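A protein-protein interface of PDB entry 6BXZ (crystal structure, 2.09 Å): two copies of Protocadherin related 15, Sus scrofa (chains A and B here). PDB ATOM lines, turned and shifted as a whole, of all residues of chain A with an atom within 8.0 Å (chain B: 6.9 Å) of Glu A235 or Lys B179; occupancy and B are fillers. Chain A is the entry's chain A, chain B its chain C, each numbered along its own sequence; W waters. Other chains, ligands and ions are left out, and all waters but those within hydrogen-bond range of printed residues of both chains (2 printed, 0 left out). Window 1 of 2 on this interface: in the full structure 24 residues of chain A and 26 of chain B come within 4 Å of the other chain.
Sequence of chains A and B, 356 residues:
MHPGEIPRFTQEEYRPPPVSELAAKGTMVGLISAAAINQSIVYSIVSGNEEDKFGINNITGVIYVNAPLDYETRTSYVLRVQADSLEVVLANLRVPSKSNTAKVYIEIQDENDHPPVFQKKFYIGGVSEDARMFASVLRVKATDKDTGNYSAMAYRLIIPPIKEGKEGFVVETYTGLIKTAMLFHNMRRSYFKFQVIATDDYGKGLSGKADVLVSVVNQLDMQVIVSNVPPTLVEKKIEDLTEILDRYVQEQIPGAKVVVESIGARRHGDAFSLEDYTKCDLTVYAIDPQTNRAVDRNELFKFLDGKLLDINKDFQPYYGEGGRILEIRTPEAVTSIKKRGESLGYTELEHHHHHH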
ATOM      1  N   VAL A 229     -37.953  17.102 -21.164  1.00  0.00           N
ATOM      2  CA  VAL A 229     -38.013  15.767 -20.567  1.00  0.00           C
ATOM      3  C   VAL A 229     -36.758  15.523 -19.714  1.00  0.00           C
ATOM      4  O   VAL A 229     -35.739  16.208 -19.916  1.00  0.00           O
ATOM      5  CB  VAL A 229     -38.161  14.663 -21.650  1.00  0.00           C
ATOM      6  CG1 VAL A 229     -39.522  14.773 -22.303  1.00  0.00           C
ATOM      7  CG2 VAL A 229     -36.983  14.671 -22.642  1.00  0.00           C
ATOM      8  N   PRO A 230     -36.835  14.572 -18.768  1.00  0.00           N
ATOM      9  CA  PRO A 230     -35.680  14.342 -17.878  1.00  0.00           C
ATOM     10  C   PRO A 230     -34.448  13.768 -18.603  1.00  0.00           C
ATOM     11  O   PRO A 230     -34.570  13.106 -19.642  1.00  0.00           O
ATOM     12  CB  PRO A 230     -36.211  13.370 -16.803  1.00  0.00           C
ATOM     13  CG  PRO A 230     -37.685  13.334 -16.978  1.00  0.00           C
ATOM     14  CD  PRO A 230     -37.999  13.740 -18.389  1.00  0.00           C
ATOM     15  N   PRO A 231     -33.249  14.061 -18.083  1.00  0.00           N
ATOM     16  CA  PRO A 231     -32.046  13.597 -18.745  1.00  0.00           C
ATOM     17  C   PRO A 231     -31.954  12.059 -18.808  1.00  0.00           C
ATOM     18  O   PRO A 231     -31.302  11.554 -19.707  1.00  0.00           O
ATOM     19  CB  PRO A 231     -30.913  14.189 -17.900  1.00  0.00           C
ATOM     20  CG  PRO A 231     -31.535  14.550 -16.608  1.00  0.00           C
ATOM     21  CD  PRO A 231     -32.960  14.867 -16.896  1.00  0.00           C
ATOM     22  N   THR A 232     -32.577  11.372 -17.857  1.00  0.00           N
ATOM     23  CA  THR A 232     -32.620   9.919 -17.879  1.00  0.00           C
ATOM     24  C   THR A 232     -33.362   9.344 -19.092  1.00  0.00           C
ATOM     25  O   THR A 232     -32.969   8.310 -19.625  1.00  0.00           O
ATOM     26  CB  THR A 232     -33.200   9.355 -16.580  1.00  0.00           C
ATOM     27  OG1 THR A 232     -34.429   9.989 -16.324  1.00  0.00           O
ATOM     28  CG2 THR A 232     -32.241   9.640 -15.432  1.00  0.00           C
ATOM     29  N   LEU A 233     -34.403  10.043 -19.548  1.00  0.00           N
ATOM     30  CA  LEU A 233     -35.113   9.616 -20.754  1.00  0.00           C
ATOM     31  C   LEU A 233     -34.218   9.827 -21.996  1.00  0.00           C
ATOM     32  O   LEU A 233     -34.055   8.933 -22.827  1.00  0.00           O
ATOM     33  CB  LEU A 233     -36.444  10.371 -20.877  1.00  0.00           C
ATOM     34  CG  LEU A 233     -37.327  10.007 -22.079  1.00  0.00           C
ATOM     35  CD1 LEU A 233     -37.578   8.499 -22.110  1.00  0.00           C
ATOM     36  CD2 LEU A 233     -38.674  10.737 -22.042  1.00  0.00           C
ATOM     37  N   VAL A 234     -33.615  11.005 -22.093  1.00  0.00           N
ATOM     38  CA  VAL A 234     -32.724  11.329 -23.208  1.00  0.00           C
ATOM     39  C   VAL A 234     -31.577  10.323 -23.284  1.00  0.00           C
ATOM     40  O   VAL A 234     -31.228   9.822 -24.379  1.00  0.00           O
ATOM     41  CB  VAL A 234     -32.222  12.806 -23.128  1.00  0.00           C
ATOM     42  CG1 VAL A 234     -31.214  13.131 -24.213  1.00  0.00           C
ATOM     43  CG2 VAL A 234     -33.385  13.784 -23.224  1.00  0.00           C
ATOM     44  N   GLU A 235     -30.993  10.008 -22.129  1.00  0.00           N
ATOM     45  CA  GLU A 235     -29.842   9.099 -22.092  1.00  0.00           C
ATOM     46  C   GLU A 235     -30.235   7.683 -22.532  1.00  0.00           C
ATOM     47  O   GLU A 235     -29.472   7.061 -23.227  1.00  0.00           O
ATOM     48  CB  GLU A 235     -29.209   9.036 -20.698  1.00  0.00           C
ATOM     49  CG  GLU A 235     -27.863   8.313 -20.654  1.00  0.00           C
ATOM     50  CD  GLU A 235     -27.953   6.821 -20.429  1.00  0.00           C
ATOM     51  OE1 GLU A 235     -29.000   6.288 -19.995  1.00  0.00           O
ATOM     52  OE2 GLU A 235     -26.931   6.156 -20.672  1.00  0.00           O
ATOM     53  N   LYS A 236     -31.406   7.210 -22.118  1.00  0.00           N
ATOM     54  CA  LYS A 236     -31.868   5.893 -22.527  1.00  0.00           C
ATOM     55  C   LYS A 236     -32.005   5.771 -24.063  1.00  0.00           C
ATOM     56  O   LYS A 236     -31.736   4.743 -24.599  1.00  0.00           O
ATOM     57  CB  LYS A 236     -33.190   5.520 -21.870  1.00  0.00           C
ATOM     58  CG  LYS A 236     -33.022   4.866 -20.517  1.00  0.00           C
ATOM     59  CD  LYS A 236     -34.375   4.540 -19.866  1.00  0.00           C
ATOM     60  CE  LYS A 236     -34.388   4.728 -18.336  1.00  0.00           C
ATOM     61  NZ  LYS A 236     -33.072   4.468 -17.630  1.00  0.00           N
ATOM     62  N   LYS A 237     -32.402   6.840 -24.726  1.00  0.00           N
ATOM     63  CA  LYS A 237     -32.689   6.851 -26.148  1.00  0.00           C
ATOM     64  C   LYS A 237     -31.590   7.509 -26.988  1.00  0.00           C
ATOM     65  O   LYS A 237     -31.787   7.721 -28.196  1.00  0.00           O
ATOM     66  CB  LYS A 237     -34.000   7.631 -26.376  1.00  0.00           C
ATOM     67  CG  LYS A 237     -35.213   7.122 -25.611  1.00  0.00           C
ATOM     68  CD  LYS A 237     -35.541   5.688 -25.960  1.00  0.00           C
ATOM     69  CE  LYS A 237     -36.919   5.334 -25.390  1.00  0.00           C
ATOM     70  NZ  LYS A 237     -37.206   3.922 -25.842  1.00  0.00           N
ATOM     71  N   ILE A 238     -30.433   7.778 -26.386  1.00  0.00           N
ATOM     72  CA  ILE A 238     -29.454   8.678 -26.988  1.00  0.00           C
ATOM     73  C   ILE A 238     -28.943   8.201 -28.362  1.00  0.00           C
ATOM     74  O   ILE A 238     -28.667   9.020 -29.224  1.00  0.00           O
ATOM     75  CB  ILE A 238     -28.289   9.023 -26.016  1.00  0.00           C
ATOM     76  CG1 ILE A 238     -27.489  10.226 -26.500  1.00  0.00           C
ATOM     77  CG2 ILE A 238     -27.358   7.846 -25.787  1.00  0.00           C
ATOM     78  CD1 ILE A 238     -28.330  11.466 -26.696  1.00  0.00           C
ATOM     79  N   GLU A 239     -28.885   6.904 -28.587  1.00  0.00           N
ATOM     80  CA  GLU A 239     -28.367   6.389 -29.859  1.00  0.00           C
ATOM     81  C   GLU A 239     -29.301   6.749 -31.019  1.00  0.00           C
ATOM     82  O   GLU A 239     -28.837   7.175 -32.058  1.00  0.00           O
ATOM     83  CB  GLU A 239     -28.180   4.865 -29.842  1.00  0.00           C
ATOM     84  CG  GLU A 239     -27.162   4.347 -28.851  1.00  0.00           C
ATOM     85  CD  GLU A 239     -25.768   4.882 -29.088  1.00  0.00           C
ATOM     86  OE1 GLU A 239     -25.150   4.514 -30.128  1.00  0.00           O
ATOM     87  OE2 GLU A 239     -25.277   5.674 -28.240  1.00  0.00           O
ATOM     88  N   ASP A 240     -30.610   6.553 -30.832  1.00  0.00           N
ATOM     89  CA  ASP A 240     -31.589   6.897 -31.843  1.00  0.00           C
ATOM     90  C   ASP A 240     -31.705   8.423 -32.005  1.00  0.00           C
ATOM     91  O   ASP A 240     -31.842   8.908 -33.116  1.00  0.00           O
ATOM     92  CB  ASP A 240     -32.940   6.327 -31.495  1.00  0.00           C
ATOM     93  CG  ASP A 240     -33.037   4.820 -31.765  1.00  0.00           C
ATOM     94  OD1 ASP A 240     -32.375   4.232 -32.618  1.00  0.00           O
ATOM     95  OD2 ASP A 240     -33.788   4.169 -31.090  1.00  0.00           O
ATOM     96  N   LEU A 241     -31.661   9.164 -30.909  1.00  0.00           N
ATOM     97  CA  LEU A 241     -31.701  10.619 -31.010  1.00  0.00           C
ATOM     98  C   LEU A 241     -30.496  11.169 -31.782  1.00  0.00           C
ATOM     99  O   LEU A 241     -30.658  12.033 -32.661  1.00  0.00           O
ATOM    100  CB  LEU A 241     -31.783  11.261 -29.631  1.00  0.00           C
ATOM    101  CG  LEU A 241     -33.007  10.867 -28.806  1.00  0.00           C
ATOM    102  CD1 LEU A 241     -32.862  11.508 -27.435  1.00  0.00           C
ATOM    103  CD2 LEU A 241     -34.299  11.249 -29.494  1.00  0.00           C
ATOM    104  N   VAL A 260     -22.251  13.645 -28.820  1.00  0.00           N
ATOM    105  CA  VAL A 260     -22.792  14.068 -27.536  1.00  0.00           C
ATOM    106  C   VAL A 260     -21.674  14.267 -26.526  1.00  0.00           C
ATOM    107  O   VAL A 260     -21.024  13.338 -26.175  1.00  0.00           O
ATOM    108  CB  VAL A 260     -23.773  12.994 -27.012  1.00  0.00           C
ATOM    109  CG1 VAL A 260     -24.237  13.329 -25.603  1.00  0.00           C
ATOM    110  CG2 VAL A 260     -24.959  12.914 -27.969  1.00  0.00           C
ATOM    111  N   ILE A 263     -25.041  14.877 -21.079  1.00  0.00           N
ATOM    112  CA  ILE A 263     -26.480  14.860 -20.889  1.00  0.00           C
ATOM    113  C   ILE A 263     -26.669  15.175 -19.429  1.00  0.00           C
ATOM    114  O   ILE A 263     -26.075  14.519 -18.586  1.00  0.00           O
ATOM    115  CB  ILE A 263     -27.077  13.459 -21.162  1.00  0.00           C
ATOM    116  CG1 ILE A 263     -26.607  12.941 -22.526  1.00  0.00           C
ATOM    117  CG2 ILE A 263     -28.611  13.525 -21.081  1.00  0.00           C
ATOM    118  CD1 ILE A 263     -27.145  11.554 -22.926  1.00  0.00           C
ATOM    119  N   GLY A 264     -27.424  16.218 -19.121  1.00  0.00           N
ATOM    120  CA  GLY A 264     -27.588  16.676 -17.749  1.00  0.00           C
ATOM    121  C   GLY A 264     -28.902  17.312 -17.499  1.00  0.00           C
ATOM    122  O   GLY A 264     -29.681  17.516 -18.436  1.00  0.00           O
ATOM    123  N   CYS A 280     -33.889  18.738 -19.550  1.00  0.00           N
ATOM    124  CA  CYS A 280     -32.594  18.195 -19.963  1.00  0.00           C
ATOM    125  C   CYS A 280     -31.824  19.156 -20.845  1.00  0.00           C
ATOM    126  O   CYS A 280     -32.367  19.725 -21.809  1.00  0.00           O
ATOM    127  CB  CYS A 280     -32.786  16.873 -20.645  1.00  0.00           C
ATOM    128  SG  CYS A 280     -31.297  16.172 -21.408  1.00  0.00           S
ATOM    129  N   LEU A 282     -28.756  18.827 -23.380  1.00  0.00           N
ATOM    130  CA  LEU A 282     -27.992  17.872 -24.189  1.00  0.00           C
ATOM    131  C   LEU A 282     -26.926  18.681 -24.935  1.00  0.00           C
ATOM    132  O   LEU A 282     -27.253  19.452 -25.800  1.00  0.00           O
ATOM    133  CB  LEU A 282     -28.937  17.133 -25.139  1.00  0.00           C
ATOM    134  CG  LEU A 282     -28.347  16.250 -26.225  1.00  0.00           C
ATOM    135  CD1 LEU A 282     -27.450  15.204 -25.630  1.00  0.00           C
ATOM    136  CD2 LEU A 282     -29.469  15.563 -27.007  1.00  0.00           C
ATOM    137  N   TYR A 319     -39.580  10.942 -27.023  1.00  0.00           N
ATOM    138  CA  TYR A 319     -39.866  11.873 -25.938  1.00  0.00           C
ATOM    139  C   TYR A 319     -41.257  11.661 -25.352  1.00  0.00           C
ATOM    140  O   TYR A 319     -41.484  12.069 -24.224  1.00  0.00           O
ATOM    141  CB  TYR A 319     -39.723  13.322 -26.427  1.00  0.00           C
ATOM    142  CG  TYR A 319     -38.327  13.876 -26.405  1.00  0.00           C
ATOM    143  CD1 TYR A 319     -37.188  13.041 -26.325  1.00  0.00           C
ATOM    144  CD2 TYR A 319     -38.119  15.242 -26.471  1.00  0.00           C
ATOM    145  CE1 TYR A 319     -35.929  13.563 -26.307  1.00  0.00           C
ATOM    146  CE2 TYR A 319     -36.846  15.760 -26.473  1.00  0.00           C
ATOM    147  CZ  TYR A 319     -35.751  14.925 -26.375  1.00  0.00           C
ATOM    148  OH  TYR A 319     -34.480  15.468 -26.325  1.00  0.00           O
ATOM    149  N   VAL B 127     -18.960   7.245  -5.522  1.00  0.00           N
ATOM    150  CA  VAL B 127     -18.952   8.290  -6.494  1.00  0.00           C
ATOM    151  C   VAL B 127     -18.235   9.482  -5.883  1.00  0.00           C
ATOM    152  O   VAL B 127     -18.369   9.791  -4.704  1.00  0.00           O
ATOM    153  CB  VAL B 127     -20.378   8.752  -6.918  1.00  0.00           C
ATOM    154  CG1 VAL B 127     -21.081   7.641  -7.579  1.00  0.00           C
ATOM    155  CG2 VAL B 127     -21.249   9.168  -5.757  1.00  0.00           C
ATOM    156  N   MET B 133     -22.373  13.231 -15.149  1.00  0.00           N
ATOM    157  CA  MET B 133     -23.653  12.539 -15.297  1.00  0.00           C
ATOM    158  C   MET B 133     -23.455  11.245 -16.095  1.00  0.00           C
ATOM    159  O   MET B 133     -22.791  11.237 -17.156  1.00  0.00           O
ATOM    160  CB  MET B 133     -24.659  13.421 -16.041  1.00  0.00           C
ATOM    161  CG  MET B 133     -25.216  14.573 -15.233  1.00  0.00           C
ATOM    162  SD  MET B 133     -26.427  14.016 -14.015  1.00  0.00           S
ATOM    163  CE  MET B 133     -27.814  13.522 -14.999  1.00  0.00           C
ATOM    164  N   PHE B 134     -24.089  10.192 -15.624  1.00  0.00           N
ATOM    165  CA  PHE B 134     -24.048   8.875 -16.239  1.00  0.00           C
ATOM    166  C   PHE B 134     -22.656   8.201 -16.186  1.00  0.00           C
ATOM    167  O   PHE B 134     -22.376   7.322 -16.971  1.00  0.00           O
ATOM    168  CB  PHE B 134     -24.680   8.916 -17.626  1.00  0.00           C
ATOM    169  CG  PHE B 134     -26.096   9.450 -17.590  1.00  0.00           C
ATOM    170  CD1 PHE B 134     -27.119   8.678 -17.056  1.00  0.00           C
ATOM    171  CD2 PHE B 134     -26.394  10.733 -18.057  1.00  0.00           C
ATOM    172  CE1 PHE B 134     -28.419   9.171 -16.978  1.00  0.00           C
ATOM    173  CE2 PHE B 134     -27.699  11.232 -18.000  1.00  0.00           C
ATOM    174  CZ  PHE B 134     -28.709  10.430 -17.442  1.00  0.00           C
ATOM    175  N   ALA B 135     -21.826   8.605 -15.211  1.00  0.00           N
ATOM    176  CA  ALA B 135     -20.544   7.938 -14.926  1.00  0.00           C
ATOM    177  C   ALA B 135     -20.860   6.538 -14.378  1.00  0.00           C
ATOM    178  O   ALA B 135     -21.827   6.351 -13.603  1.00  0.00           O
ATOM    179  CB  ALA B 135     -19.762   8.704 -13.876  1.00  0.00           C
ATOM    180  N   SER B 136     -20.035   5.574 -14.745  1.00  0.00           N
ATOM    181  CA  SER B 136     -20.196   4.225 -14.291  1.00  0.00           C
ATOM    182  C   SER B 136     -19.877   4.171 -12.810  1.00  0.00           C
ATOM    183  O   SER B 136     -18.950   4.817 -12.350  1.00  0.00           O
ATOM    184  CB  SER B 136     -19.243   3.286 -15.026  1.00  0.00           C
ATOM    185  OG  SER B 136     -19.612   3.335 -16.375  1.00  0.00           O
ATOM    186  N   VAL B 137     -20.676   3.421 -12.062  1.00  0.00           N
ATOM    187  CA  VAL B 137     -20.470   3.248 -10.643  1.00  0.00           C
ATOM    188  C   VAL B 137     -20.000   1.811 -10.425  1.00  0.00           C
ATOM    189  O   VAL B 137     -18.886   1.592  -9.941  1.00  0.00           O
ATOM    190  CB  VAL B 137     -21.739   3.554  -9.842  1.00  0.00           C
ATOM    191  CG1 VAL B 137     -21.505   3.306  -8.357  1.00  0.00           C
ATOM    192  CG2 VAL B 137     -22.170   4.984 -10.087  1.00  0.00           C
ATOM    193  N   LEU B 138     -20.842   0.847 -10.772  1.00  0.00           N
ATOM    194  CA  LEU B 138     -20.446  -0.564 -10.726  1.00  0.00           C
ATOM    195  C   LEU B 138     -21.368  -1.393 -11.605  1.00  0.00           C
ATOM    196  O   LEU B 138     -22.433  -0.937 -12.010  1.00  0.00           O
ATOM    197  CB  LEU B 138     -20.472  -1.067  -9.278  1.00  0.00           C
ATOM    198  CG  LEU B 138     -21.796  -1.067  -8.519  1.00  0.00           C
ATOM    199  CD1 LEU B 138     -22.609  -2.323  -8.756  1.00  0.00           C
ATOM    200  CD2 LEU B 138     -21.446  -1.058  -7.040  1.00  0.00           C
ATOM    201  N   LEU B 157     -33.622  -0.873 -10.436  1.00  0.00           N
ATOM    202  CA  LEU B 157     -33.269  -0.369  -9.114  1.00  0.00           C
ATOM    203  C   LEU B 157     -34.515  -0.023  -8.306  1.00  0.00           C
ATOM    204  O   LEU B 157     -35.508   0.436  -8.839  1.00  0.00           O
ATOM    205  CB  LEU B 157     -32.383   0.871  -9.251  1.00  0.00           C
ATOM    206  CG  LEU B 157     -31.062   0.635 -10.005  1.00  0.00           C
ATOM    207  CD1 LEU B 157     -30.201   1.901  -9.998  1.00  0.00           C
ATOM    208  CD2 LEU B 157     -30.278  -0.555  -9.448  1.00  0.00           C
ATOM    209  N   GLY B 168     -31.046   9.774  -8.739  1.00  0.00           N
ATOM    210  CA  GLY B 168     -29.867   9.242  -8.022  1.00  0.00           C
ATOM    211  C   GLY B 168     -28.951   8.448  -8.968  1.00  0.00           C
ATOM    212  O   GLY B 168     -27.856   8.918  -9.324  1.00  0.00           O
ATOM    213  N   PHE B 169     -29.416   7.239  -9.309  1.00  0.00           N
ATOM    214  CA  PHE B 169     -28.721   6.266 -10.152  1.00  0.00           C
ATOM    215  C   PHE B 169     -29.721   5.587 -11.075  1.00  0.00           C
ATOM    216  O   PHE B 169     -30.920   5.548 -10.780  1.00  0.00           O
ATOM    217  CB  PHE B 169     -28.058   5.197  -9.274  1.00  0.00           C
ATOM    218  CG  PHE B 169     -27.152   5.779  -8.225  1.00  0.00           C
ATOM    219  CD1 PHE B 169     -27.672   6.132  -6.991  1.00  0.00           C
ATOM    220  CD2 PHE B 169     -25.830   6.070  -8.504  1.00  0.00           C
ATOM    221  CE1 PHE B 169     -26.884   6.735  -6.028  1.00  0.00           C
ATOM    222  CE2 PHE B 169     -25.040   6.668  -7.545  1.00  0.00           C
ATOM    223  CZ  PHE B 169     -25.564   6.988  -6.292  1.00  0.00           C
ATOM    224  N   VAL B 170     -29.212   5.058 -12.185  1.00  0.00           N
ATOM    225  CA  VAL B 170     -29.970   4.238 -13.080  1.00  0.00           C
ATOM    226  C   VAL B 170     -29.157   2.996 -13.342  1.00  0.00           C
ATOM    227  O   VAL B 170     -27.943   2.980 -13.103  1.00  0.00           O
ATOM    228  CB  VAL B 170     -30.301   4.913 -14.445  1.00  0.00           C
ATOM    229  CG1 VAL B 170     -31.343   6.012 -14.254  1.00  0.00           C
ATOM    230  CG2 VAL B 170     -29.043   5.391 -15.183  1.00  0.00           C
ATOM    231  N   VAL B 171     -29.835   1.967 -13.842  1.00  0.00           N
ATOM    232  CA  VAL B 171     -29.172   0.743 -14.267  1.00  0.00           C
ATOM    233  C   VAL B 171     -29.548   0.464 -15.712  1.00  0.00           C
ATOM    234  O   VAL B 171     -30.687   0.624 -16.098  1.00  0.00           O
ATOM    235  CB  VAL B 171     -29.472  -0.462 -13.337  1.00  0.00           C
ATOM    236  CG1 VAL B 171     -30.940  -0.927 -13.407  1.00  0.00           C
ATOM    237  CG2 VAL B 171     -28.519  -1.622 -13.653  1.00  0.00           C
ATOM    238  N   GLU B 172     -28.565   0.087 -16.508  1.00  0.00           N
ATOM    239  CA  GLU B 172     -28.811  -0.377 -17.869  1.00  0.00           C
ATOM    240  C   GLU B 172     -29.557  -1.702 -17.749  1.00  0.00           C
ATOM    241  O   GLU B 172     -29.099  -2.613 -17.081  1.00  0.00           O
ATOM    242  CB  GLU B 172     -27.502  -0.548 -18.617  1.00  0.00           C
ATOM    243  CG  GLU B 172     -26.748   0.760 -18.819  1.00  0.00           C
ATOM    244  CD  GLU B 172     -25.555   0.651 -19.789  1.00  0.00           C
ATOM    245  OE1 GLU B 172     -25.163  -0.479 -20.170  1.00  0.00           O
ATOM    246  OE2 GLU B 172     -24.983   1.708 -20.150  1.00  0.00           O
ATOM    247  N   GLY B 176     -26.644  -4.627 -16.676  1.00  0.00           N
ATOM    248  CA  GLY B 176     -26.373  -4.498 -15.252  1.00  0.00           C
ATOM    249  C   GLY B 176     -25.466  -3.341 -14.831  1.00  0.00           C
ATOM    250  O   GLY B 176     -25.101  -3.284 -13.653  1.00  0.00           O
ATOM    251  N   LEU B 177     -25.118  -2.433 -15.738  1.00  0.00           N
ATOM    252  CA  LEU B 177     -24.260  -1.309 -15.389  1.00  0.00           C
ATOM    253  C   LEU B 177     -25.030  -0.229 -14.630  1.00  0.00           C
ATOM    254  O   LEU B 177     -25.990   0.344 -15.154  1.00  0.00           O
ATOM    255  CB  LEU B 177     -23.591  -0.706 -16.636  1.00  0.00           C
ATOM    256  CG  LEU B 177     -22.587   0.435 -16.413  1.00  0.00           C
ATOM    257  CD1 LEU B 177     -21.432  -0.006 -15.521  1.00  0.00           C
ATOM    258  CD2 LEU B 177     -22.080   1.018 -17.728  1.00  0.00           C
ATOM    259  N   ILE B 178     -24.612   0.063 -13.404  1.00  0.00           N
ATOM    260  CA  ILE B 178     -25.240   1.118 -12.619  1.00  0.00           C
ATOM    261  C   ILE B 178     -24.460   2.404 -12.885  1.00  0.00           C
ATOM    262  O   ILE B 178     -23.222   2.393 -12.787  1.00  0.00           O
ATOM    263  CB  ILE B 178     -25.252   0.779 -11.113  1.00  0.00           C
ATOM    264  CG1 ILE B 178     -26.170  -0.423 -10.874  1.00  0.00           C
ATOM    265  CG2 ILE B 178     -25.686   1.995 -10.295  1.00  0.00           C
ATOM    266  CD1 ILE B 178     -26.162  -1.009  -9.472  1.00  0.00           C
ATOM    267  N   LYS B 179     -25.169   3.484 -13.222  1.00  0.00           N
ATOM    268  CA  LYS B 179     -24.551   4.785 -13.575  1.00  0.00           C
ATOM    269  C   LYS B 179     -25.171   5.880 -12.728  1.00  0.00           C
ATOM    270  O   LYS B 179     -26.304   5.718 -12.249  1.00  0.00           O
ATOM    271  CB  LYS B 179     -24.790   5.094 -15.058  1.00  0.00           C
ATOM    272  CG  LYS B 179     -24.240   4.049 -15.994  1.00  0.00           C
ATOM    273  CD  LYS B 179     -24.417   4.404 -17.470  1.00  0.00           C
ATOM    274  CE  LYS B 179     -25.853   4.245 -17.860  1.00  0.00           C
ATOM    275  NZ  LYS B 179     -25.984   4.241 -19.334  1.00  0.00           N
ATOM    276  N   THR B 180     -24.470   7.018 -12.602  1.00  0.00           N
ATOM    277  CA  THR B 180     -25.008   8.176 -11.894  1.00  0.00           C
ATOM    278  C   THR B 180     -26.147   8.844 -12.700  1.00  0.00           C
ATOM    279  O   THR B 180     -26.149   8.846 -13.965  1.00  0.00           O
ATOM    280  CB  THR B 180     -23.937   9.246 -11.584  1.00  0.00           C
ATOM    281  OG1 THR B 180     -23.445   9.806 -12.786  1.00  0.00           O
ATOM    282  CG2 THR B 180     -22.764   8.676 -10.816  1.00  0.00           C
ATOM    283  N   ALA B 181     -27.139   9.401 -11.987  1.00  0.00           N
ATOM    284  CA  ALA B 181     -28.192  10.136 -12.647  1.00  0.00           C
ATOM    285  C   ALA B 181     -28.416  11.512 -12.052  1.00  0.00           C
ATOM    286  O   ALA B 181     -29.396  12.158 -12.380  1.00  0.00           O
ATOM    287  CB  ALA B 181     -29.465   9.317 -12.664  1.00  0.00           C
ATOM    288  N   MET B 182     -27.469  11.981 -11.258  1.00  0.00           N
ATOM    289  CA  MET B 182     -27.482  13.363 -10.739  1.00  0.00           C
ATOM    290  C   MET B 182     -26.034  13.745 -10.448  1.00  0.00           C
ATOM    291  O   MET B 182     -25.171  12.845 -10.335  1.00  0.00           O
ATOM    292  CB  MET B 182     -28.310  13.434  -9.432  1.00  0.00           C
ATOM    293  CG  MET B 182     -27.765  12.538  -8.293  1.00  0.00           C
ATOM    294  SD  MET B 182     -28.956  12.679  -6.952  1.00  0.00           S
ATOM    295  CE  MET B 182     -28.081  11.948  -5.610  1.00  0.00           C
HETATM  296  O   HOH W   1     -23.313  12.865 -19.479  1.00  0.00           O
HETATM  297  O   HOH W   2     -28.685   3.839 -19.623  1.00  0.00           O
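Printed residues of chain B within 4 Å of Pro A231: Phe B134 (3.6 Å). Printed residues of chain B within 4 Å of Ile A263: Met B133 and Phe B134. Lys B179 touches just one residue of chain A: Glu A235 (2.5 Å). The nearest residue of chain A that does not touch Lys B179 is Lys A236 (6.8 Å).
Among the printed residues, pairs that only touch across the chains: Ile A263 with Met B133 (3.1 Å), Glu A235 with Phe B134 (3.6 Å), Pro A231 with Phe B134 (3.6 Å), Ile A263 with Phe B134 (3.7 Å), Thr A232 with Val B170 (3.9 Å), Thr A232 with Ala B181 (3.9 Å) and Thr A232 with Phe B134 (3.97 Å).
OE2 of Glu A235 is in salt-bridge range of NZ of Lys B179.
Water W2 bridges OE1 of Glu A235 (2.5 Å) and NZ of Lys B179 (2.7 Å). Water W1 bridges O of Met B133 (2.9 Å) and N of Ile A263 (3.1 Å).
SD of Met B133 lies close to N of Met B182, 3.6 Å away. The backbone NH of Phe B134 is in hydrogen-bond range of the side-chain hydroxyl of Thr B180, at 2.9 Å. O of Gly B168 sits at hydrogen-bond distance from N of Ala B181, at 2.8 Å. O of Val B170 is in hydrogen-bond range of N of Lys B179 (2.8 Å). NZ of Lys B179 lies within salt-bridge range of OE2 of Glu B172 (2.8 Å).
No position is printed for both chains. Of the 8 pairs that touch across the chains among the printed residues, none has its exchanged pair printed and touching as well.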
